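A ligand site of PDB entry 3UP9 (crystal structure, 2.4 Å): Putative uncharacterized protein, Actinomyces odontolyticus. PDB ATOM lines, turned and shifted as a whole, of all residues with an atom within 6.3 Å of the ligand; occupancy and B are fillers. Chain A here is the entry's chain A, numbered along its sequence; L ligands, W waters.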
ATOM      1  N   THR A  14      18.728  -9.827   1.072  1.00  0.00           N
ATOM      2  CA  THR A  14      17.343 -10.255   1.387  1.00  0.00           C
ATOM      3  C   THR A  14      16.527 -10.096   0.102  1.00  0.00           C
ATOM      4  O   THR A  14      16.860  -9.315  -0.793  1.00  0.00           O
ATOM      5  CB  THR A  14      16.735  -9.487   2.598  1.00  0.00           C
ATOM      6  OG1 THR A  14      17.064  -8.091   2.491  1.00  0.00           O
ATOM      7  CG2 THR A  14      17.242 -10.111   3.936  1.00  0.00           C
ATOM      8  N   SER A  16      13.574  -8.744  -0.988  1.00  0.00           N
ATOM      9  CA  SER A  16      12.929  -7.476  -1.399  1.00  0.00           C
ATOM     10  C   SER A  16      13.166  -6.435  -0.335  1.00  0.00           C
ATOM     11  O   SER A  16      12.896  -6.674   0.823  1.00  0.00           O
ATOM     12  CB  SER A  16      11.443  -7.656  -1.665  1.00  0.00           C
ATOM     13  OG  SER A  16      10.945  -6.508  -2.301  1.00  0.00           O
ATOM     14  N   PRO A  17      13.670  -5.265  -0.719  1.00  0.00           N
ATOM     15  CA  PRO A  17      14.074  -4.766  -2.043  1.00  0.00           C
ATOM     16  C   PRO A  17      15.437  -5.229  -2.608  1.00  0.00           C
ATOM     17  O   PRO A  17      15.695  -5.082  -3.831  1.00  0.00           O
ATOM     18  CB  PRO A  17      14.108  -3.239  -1.843  1.00  0.00           C
ATOM     19  CG  PRO A  17      14.471  -3.065  -0.404  1.00  0.00           C
ATOM     20  CD  PRO A  17      13.781  -4.211   0.314  1.00  0.00           C
ATOM     21  N   HIS A  18      16.298  -5.760  -1.736  1.00  0.00           N
ATOM     22  CA  HIS A  18      17.715  -5.832  -2.040  1.00  0.00           C
ATOM     23  C   HIS A  18      18.014  -6.699  -3.240  1.00  0.00           C
ATOM     24  O   HIS A  18      18.649  -6.238  -4.168  1.00  0.00           O
ATOM     25  CB  HIS A  18      18.514  -6.270  -0.806  1.00  0.00           C
ATOM     26  CG  HIS A  18      18.175  -5.492   0.439  1.00  0.00           C
ATOM     27  ND1 HIS A  18      17.073  -5.715   1.137  1.00  0.00           N
ATOM     28  CD2 HIS A  18      18.848  -4.436   1.077  1.00  0.00           C
ATOM     29  CE1 HIS A  18      17.026  -4.836   2.173  1.00  0.00           C
ATOM     30  NE2 HIS A  18      18.111  -4.059   2.113  1.00  0.00           N
ATOM     31  N   TYR A  45      18.962 -12.259   9.272  1.00  0.00           N
ATOM     32  CA  TYR A  45      19.945 -11.197   9.394  1.00  0.00           C
ATOM     33  C   TYR A  45      21.325 -11.701   9.806  1.00  0.00           C
ATOM     34  O   TYR A  45      22.302 -11.068   9.442  1.00  0.00           O
ATOM     35  CB  TYR A  45      19.442 -10.132  10.363  1.00  0.00           C
ATOM     36  CG  TYR A  45      18.253  -9.262   9.892  1.00  0.00           C
ATOM     37  CD1 TYR A  45      17.967  -9.114   8.538  1.00  0.00           C
ATOM     38  CD2 TYR A  45      17.482  -8.528  10.805  1.00  0.00           C
ATOM     39  CE1 TYR A  45      16.930  -8.318   8.112  1.00  0.00           C
ATOM     40  CE2 TYR A  45      16.449  -7.702  10.391  1.00  0.00           C
ATOM     41  CZ  TYR A  45      16.185  -7.594   9.042  1.00  0.00           C
ATOM     42  OH  TYR A  45      15.194  -6.773   8.568  1.00  0.00           O
ATOM     43  N   TYR A  62      21.955  -5.887   2.666  1.00  0.00           N
ATOM     44  CA  TYR A  62      20.748  -6.212   3.432  1.00  0.00           C
ATOM     45  C   TYR A  62      20.605  -5.447   4.737  1.00  0.00           C
ATOM     46  O   TYR A  62      19.563  -5.487   5.317  1.00  0.00           O
ATOM     47  CB  TYR A  62      20.702  -7.717   3.757  1.00  0.00           C
ATOM     48  CG  TYR A  62      21.477  -8.132   4.992  1.00  0.00           C
ATOM     49  CD1 TYR A  62      22.859  -8.257   4.960  1.00  0.00           C
ATOM     50  CD2 TYR A  62      20.845  -8.399   6.183  1.00  0.00           C
ATOM     51  CE1 TYR A  62      23.590  -8.628   6.083  1.00  0.00           C
ATOM     52  CE2 TYR A  62      21.560  -8.750   7.287  1.00  0.00           C
ATOM     53  CZ  TYR A  62      22.938  -8.853   7.245  1.00  0.00           C
ATOM     54  OH  TYR A  62      23.646  -9.231   8.373  1.00  0.00           O
ATOM     55  N   GLN A  63      21.669  -4.776   5.207  1.00  0.00           N
ATOM     56  CA  GLN A  63      21.704  -4.276   6.555  1.00  0.00           C
ATOM     57  C   GLN A  63      21.840  -2.732   6.644  1.00  0.00           C
ATOM     58  O   GLN A  63      22.254  -2.079   5.694  1.00  0.00           O
ATOM     59  CB  GLN A  63      22.771  -5.003   7.370  1.00  0.00           C
ATOM     60  CG  GLN A  63      24.162  -4.473   7.225  1.00  0.00           C
ATOM     61  CD  GLN A  63      25.178  -5.454   7.746  1.00  0.00           C
ATOM     62  OE1 GLN A  63      25.313  -5.612   8.950  1.00  0.00           O
ATOM     63  NE2 GLN A  63      25.906  -6.097   6.841  1.00  0.00           N
ATOM     64  N   THR A  64      21.428  -2.214   7.787  1.00  0.00           N
ATOM     65  CA  THR A  64      21.373  -0.809   8.074  1.00  0.00           C
ATOM     66  C   THR A  64      22.670  -0.498   8.786  1.00  0.00           C
ATOM     67  O   THR A  64      23.317  -1.362   9.342  1.00  0.00           O
ATOM     68  CB  THR A  64      20.140  -0.433   8.966  1.00  0.00           C
ATOM     69  OG1 THR A  64      20.238  -1.082  10.273  1.00  0.00           O
ATOM     70  CG2 THR A  64      18.780  -0.816   8.287  1.00  0.00           C
ATOM     71  N   TYR A  67      22.661  -1.449  12.600  1.00  0.00           N
ATOM     72  CA  TYR A  67      22.812  -2.877  12.777  1.00  0.00           C
ATOM     73  C   TYR A  67      24.260  -3.292  12.520  1.00  0.00           C
ATOM     74  O   TYR A  67      24.815  -4.108  13.294  1.00  0.00           O
ATOM     75  CB  TYR A  67      21.847  -3.603  11.828  1.00  0.00           C
ATOM     76  CG  TYR A  67      21.985  -5.117  11.874  1.00  0.00           C
ATOM     77  CD1 TYR A  67      22.980  -5.765  11.142  1.00  0.00           C
ATOM     78  CD2 TYR A  67      21.119  -5.880  12.641  1.00  0.00           C
ATOM     79  CE1 TYR A  67      23.103  -7.149  11.178  1.00  0.00           C
ATOM     80  CE2 TYR A  67      21.248  -7.262  12.669  1.00  0.00           C
ATOM     81  CZ  TYR A  67      22.250  -7.895  11.947  1.00  0.00           C
ATOM     82  OH  TYR A  67      22.425  -9.282  12.011  1.00  0.00           O
ATOM     83  N   LEU A  68      24.869  -2.771  11.445  1.00  0.00           N
ATOM     84  CA  LEU A  68      26.272  -3.059  11.127  1.00  0.00           C
ATOM     85  C   LEU A  68      27.204  -2.641  12.267  1.00  0.00           C
ATOM     86  O   LEU A  68      28.066  -3.400  12.658  1.00  0.00           O
ATOM     87  CB  LEU A  68      26.701  -2.397   9.795  1.00  0.00           C
ATOM     88  CG  LEU A  68      28.202  -2.460   9.402  1.00  0.00           C
ATOM     89  CD1 LEU A  68      28.645  -3.907   9.186  1.00  0.00           C
ATOM     90  CD2 LEU A  68      28.446  -1.620   8.139  1.00  0.00           C
ATOM     91  N   HIS A  86      19.076   3.090   0.454  1.00  0.00           N
ATOM     92  CA  HIS A  86      17.687   3.321   0.713  1.00  0.00           C
ATOM     93  C   HIS A  86      17.355   3.078   2.163  1.00  0.00           C
ATOM     94  O   HIS A  86      18.091   2.434   2.887  1.00  0.00           O
ATOM     95  CB  HIS A  86      16.839   2.410  -0.136  1.00  0.00           C
ATOM     96  CG  HIS A  86      16.927   0.963   0.261  1.00  0.00           C
ATOM     97  ND1 HIS A  86      17.784   0.120  -0.301  1.00  0.00           N
ATOM     98  CD2 HIS A  86      16.225   0.225   1.205  1.00  0.00           C
ATOM     99  CE1 HIS A  86      17.644  -1.104   0.262  1.00  0.00           C
ATOM    100  NE2 HIS A  86      16.679  -1.025   1.166  1.00  0.00           N
ATOM    101  N   LEU A  87      16.226   3.667   2.560  1.00  0.00           N
ATOM    102  CA  LEU A  87      15.597   3.503   3.825  1.00  0.00           C
ATOM    103  C   LEU A  87      14.318   2.698   3.655  1.00  0.00           C
ATOM    104  O   LEU A  87      13.576   2.884   2.662  1.00  0.00           O
ATOM    105  CB  LEU A  87      15.266   4.910   4.368  1.00  0.00           C
ATOM    106  CG  LEU A  87      14.523   5.058   5.669  1.00  0.00           C
ATOM    107  CD1 LEU A  87      15.509   4.699   6.775  1.00  0.00           C
ATOM    108  CD2 LEU A  87      13.999   6.501   5.793  1.00  0.00           C
ATOM    109  N   GLU A  88      14.063   1.800   4.614  1.00  0.00           N
ATOM    110  CA  GLU A  88      12.792   1.089   4.757  1.00  0.00           C
ATOM    111  C   GLU A  88      12.148   1.498   6.063  1.00  0.00           C
ATOM    112  O   GLU A  88      12.560   0.976   7.107  1.00  0.00           O
ATOM    113  CB  GLU A  88      13.014  -0.433   4.816  1.00  0.00           C
ATOM    114  CG  GLU A  88      13.340  -1.143   3.517  1.00  0.00           C
ATOM    115  CD  GLU A  88      14.173  -2.401   3.751  1.00  0.00           C
ATOM    116  OE1 GLU A  88      13.876  -3.142   4.714  1.00  0.00           O
ATOM    117  OE2 GLU A  88      15.148  -2.648   3.012  1.00  0.00           O
ATOM    118  N   LEU A  90      10.225   1.587   9.371  1.00  0.00           N
ATOM    119  CA  LEU A  90       9.771   0.519  10.236  1.00  0.00           C
ATOM    120  C   LEU A  90       8.310   0.744  10.514  1.00  0.00           C
ATOM    121  O   LEU A  90       7.852   1.899  10.677  1.00  0.00           O
ATOM    122  CB  LEU A  90      10.601   0.496  11.522  1.00  0.00           C
ATOM    123  CG  LEU A  90      10.476  -0.723  12.429  1.00  0.00           C
ATOM    124  CD1 LEU A  90      10.890  -2.055  11.739  1.00  0.00           C
ATOM    125  CD2 LEU A  90      11.235  -0.434  13.720  1.00  0.00           C
ATOM    126  N   ASP A 114      16.953  -9.374  17.732  1.00  0.00           N
ATOM    127  CA  ASP A 114      18.316  -8.798  17.631  1.00  0.00           C
ATOM    128  C   ASP A 114      18.378  -7.401  18.287  1.00  0.00           C
ATOM    129  O   ASP A 114      17.393  -6.650  18.218  1.00  0.00           O
ATOM    130  CB  ASP A 114      18.803  -8.829  16.178  1.00  0.00           C
ATOM    131  CG  ASP A 114      18.271  -7.673  15.306  1.00  0.00           C
ATOM    132  OD1 ASP A 114      18.813  -6.513  15.385  1.00  0.00           O
ATOM    133  OD2 ASP A 114      17.365  -7.934  14.488  1.00  0.00           O
ATOM    134  N   ALA A 116      19.989  -4.315  17.712  1.00  0.00           N
ATOM    135  CA  ALA A 116      19.825  -3.091  16.933  1.00  0.00           C
ATOM    136  C   ALA A 116      18.386  -2.814  16.494  1.00  0.00           C
ATOM    137  O   ALA A 116      17.923  -1.649  16.551  1.00  0.00           O
ATOM    138  CB  ALA A 116      20.706  -3.152  15.717  1.00  0.00           C
ATOM    139  N   ASN A 117      17.707  -3.859  16.014  1.00  0.00           N
ATOM    140  CA  ASN A 117      16.337  -3.753  15.496  1.00  0.00           C
ATOM    141  C   ASN A 117      15.251  -3.734  16.588  1.00  0.00           C
ATOM    142  O   ASN A 117      14.224  -3.057  16.408  1.00  0.00           O
ATOM    143  CB  ASN A 117      16.037  -4.833  14.437  1.00  0.00           C
ATOM    144  CG  ASN A 117      16.801  -4.603  13.155  1.00  0.00           C
ATOM    145  OD1 ASN A 117      16.697  -3.527  12.534  1.00  0.00           O
ATOM    146  ND2 ASN A 117      17.620  -5.559  12.802  1.00  0.00           N
ATOM    147  N   ARG A 120      15.472  -0.244  17.764  1.00  0.00           N
ATOM    148  CA  ARG A 120      14.806   0.661  16.838  1.00  0.00           C
ATOM    149  C   ARG A 120      13.229   0.609  16.936  1.00  0.00           C
ATOM    150  O   ARG A 120      12.571   1.645  16.875  1.00  0.00           O
ATOM    151  CB  ARG A 120      15.313   0.371  15.448  1.00  0.00           C
ATOM    152  CG  ARG A 120      14.582   1.066  14.323  1.00  0.00           C
ATOM    153  CD  ARG A 120      15.160   0.588  13.010  1.00  0.00           C
ATOM    154  NE  ARG A 120      14.610   1.214  11.810  1.00  0.00           N
ATOM    155  CZ  ARG A 120      14.782   0.697  10.595  1.00  0.00           C
ATOM    156  NH1 ARG A 120      15.526  -0.381  10.434  1.00  0.00           N
ATOM    157  NH2 ARG A 120      14.288   1.286   9.546  1.00  0.00           N
ATOM    158  N   ASN A 174      10.349  -4.913  10.246  1.00  0.00           N
ATOM    159  CA  ASN A 174      11.208  -4.296   9.244  1.00  0.00           C
ATOM    160  C   ASN A 174      10.669  -4.500   7.852  1.00  0.00           C
ATOM    161  O   ASN A 174      10.076  -5.582   7.520  1.00  0.00           O
ATOM    162  CB  ASN A 174      12.634  -4.886   9.335  1.00  0.00           C
ATOM    163  CG  ASN A 174      13.304  -4.644  10.697  1.00  0.00           C
ATOM    164  OD1 ASN A 174      12.968  -5.276  11.717  1.00  0.00           O
ATOM    165  ND2 ASN A 174      14.253  -3.734  10.704  1.00  0.00           N
ATOM    166  N   GLY A 175      10.892  -3.496   7.007  1.00  0.00           N
ATOM    167  CA  GLY A 175      10.419  -3.533   5.590  1.00  0.00           C
ATOM    168  C   GLY A 175      10.642  -4.812   4.818  1.00  0.00           C
ATOM    169  O   GLY A 175       9.689  -5.357   4.279  1.00  0.00           O
ATOM    170  N   ASN A 176      11.873  -5.324   4.791  1.00  0.00           N
ATOM    171  CA  ASN A 176      12.205  -6.556   4.067  1.00  0.00           C
ATOM    172  C   ASN A 176      11.275  -7.693   4.438  1.00  0.00           C
ATOM    173  O   ASN A 176      10.918  -8.432   3.561  1.00  0.00           O
ATOM    174  CB  ASN A 176      13.676  -6.994   4.229  1.00  0.00           C
ATOM    175  CG  ASN A 176      14.038  -7.407   5.638  1.00  0.00           C
ATOM    176  OD1 ASN A 176      14.146  -6.567   6.533  1.00  0.00           O
ATOM    177  ND2 ASN A 176      14.231  -8.709   5.849  1.00  0.00           N
ATOM    178  N   ALA A 200      18.827   4.696   9.814  1.00  0.00           N
ATOM    179  CA  ALA A 200      18.751   3.293   9.383  1.00  0.00           C
ATOM    180  C   ALA A 200      18.771   3.098   7.873  1.00  0.00           C
ATOM    181  O   ALA A 200      17.947   2.339   7.316  1.00  0.00           O
ATOM    182  CB  ALA A 200      17.545   2.579   9.999  1.00  0.00           C
ATOM    183  N   VAL A 201      19.753   3.719   7.220  1.00  0.00           N
ATOM    184  CA  VAL A 201      19.946   3.525   5.782  1.00  0.00           C
ATOM    185  C   VAL A 201      20.687   2.192   5.524  1.00  0.00           C
ATOM    186  O   VAL A 201      21.603   1.781   6.241  1.00  0.00           O
ATOM    187  CB  VAL A 201      20.697   4.708   5.139  1.00  0.00           C
ATOM    188  CG1 VAL A 201      19.867   5.996   5.259  1.00  0.00           C
ATOM    189  CG2 VAL A 201      22.085   4.892   5.750  1.00  0.00           C
ATOM    190  N   ASN A 202      20.287   1.560   4.422  1.00  0.00           N
ATOM    191  CA  ASN A 202      20.809   0.274   3.991  1.00  0.00           C
ATOM    192  C   ASN A 202      22.051   0.393   3.107  1.00  0.00           C
ATOM    193  O   ASN A 202      22.059   1.117   2.133  1.00  0.00           O
ATOM    194  CB  ASN A 202      19.731  -0.485   3.205  1.00  0.00           C
ATOM    195  CG  ASN A 202      18.653  -1.045   4.078  1.00  0.00           C
ATOM    196  OD1 ASN A 202      18.635  -2.250   4.363  1.00  0.00           O
ATOM    197  ND2 ASN A 202      17.709  -0.178   4.474  1.00  0.00           N
HETATM  198  N1  LIG L   1      16.177  -4.158   5.497  1.00  0.00           N
HETATM  199  C1  LIG L   1      16.139  -3.873   6.942  1.00  0.00           C
HETATM  200  C2  LIG L   1      15.792  -2.440   7.269  1.00  0.00           C
HETATM  201  O1  LIG L   1      16.166  -1.514   6.494  1.00  0.00           O
HETATM  202  O2  LIG L   1      15.144  -2.246   8.305  1.00  0.00           O
HETATM  203  C3  LIG L   1      17.476  -4.189   7.564  1.00  0.00           C
HETATM  204  C4  LIG L   1      17.505  -4.059   9.118  1.00  0.00           C
HETATM  205 SE1  LIG L   1      19.266  -4.458   9.787  1.00  0.00          SE
HETATM  206  C5  LIG L   1      19.627  -6.287   9.067  1.00  0.00           C
HETATM  207  O   HOH W   1      17.053  -6.603   4.884  1.00  0.00           O
HETATM  208  O   HOH W   2      12.451  -1.385   8.201  1.00  0.00           O
HETATM  209  O   HOH W   3      15.489   1.132   7.040  1.00  0.00           O
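Merely in contact with the ligand: Thr 64 (3.2 Å), Tyr 45 (3.3 Å), Tyr 62 (3.3 Å), Tyr 67 (3.4 Å), His 18 (3.5 Å), Asn 117 (3.6 Å) and Gln 63 (3.8 Å).
Hydrophobic or aromatic side chains within 4 Å of the ligand: His 18, Tyr 45, Tyr 62 and Tyr 67.
Of the 24 residues printed, 12 come within 4 Å of the ligand.
OE1 of Glu 88 lies within salt-bridge range of N1 of the ligand, at 2.6 Å.
An oxygen (O2) of the ligand is in salt-bridge range of the guanidinium group (NH1) of Arg 120 (2.9 Å).
The side-chain amide nitrogen (ND2) of Asn 202 lies within hydrogen-bond range of an oxygen (O1) of the ligand.
O2 of the ligand is in hydrogen-bond range of ND2 of Asn 174, 3.0 Å away.
OD1 of Asn 176 sits at hydrogen-bond distance from N1 of the ligand, 3.3 Å away.
The side-chain carboxylate of Glu 88 lies within hydrogen-bond range of the backbone NH of Asn 176 (3.0 Å).
OE2 of Glu 88 is in hydrogen-bond range of NE2 of His 86, at 2.9 Å.
The backbone NH (N) of Asn 202 lies within hydrogen-bond range of the backbone carbonyl oxygen (O) of His 86, 2.8 Å away.
The side-chain hydroxyl (OG1) of Thr 64 lies close to the backbone NH (N) of Tyr 67 (3.4 Å).
The backbone carbonyl oxygen (O) of Tyr 45 lies within hydrogen-bond range of the side-chain hydroxyl (OH) of Tyr 62, at 2.5 Å.
OH of Tyr 67 is in hydrogen-bond range of O of Tyr 45, at 3.1 Å.
A ring nitrogen (NE2) of His 18 is in hydrogen-bond range of a ring nitrogen (NE2) of His 86.
The side-chain amide nitrogen (ND2) of Asn 117 sits at hydrogen-bond distance from the side-chain carboxylate (OD2) of Asp 114.
Water W1 lies within hydrogen-bond range of a nitrogen (N1) of the ligand (2.7 Å), the backbone carbonyl oxygen of Tyr 62 (2.8 Å), the side-chain hydroxyl of Thr 14 (2.8 Å) and the side-chain amide oxygen of Asn 176 (3.3 Å).
Water W3 lies within hydrogen-bond range of O of Ala 200, NH2 of Arg 120, O1 of the ligand and N of Glu 88.
Water W2 lies within hydrogen-bond range of the backbone carbonyl oxygen (O) of Glu 88, an oxygen (O2) of the ligand and the backbone NH (N) of Gly 175.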
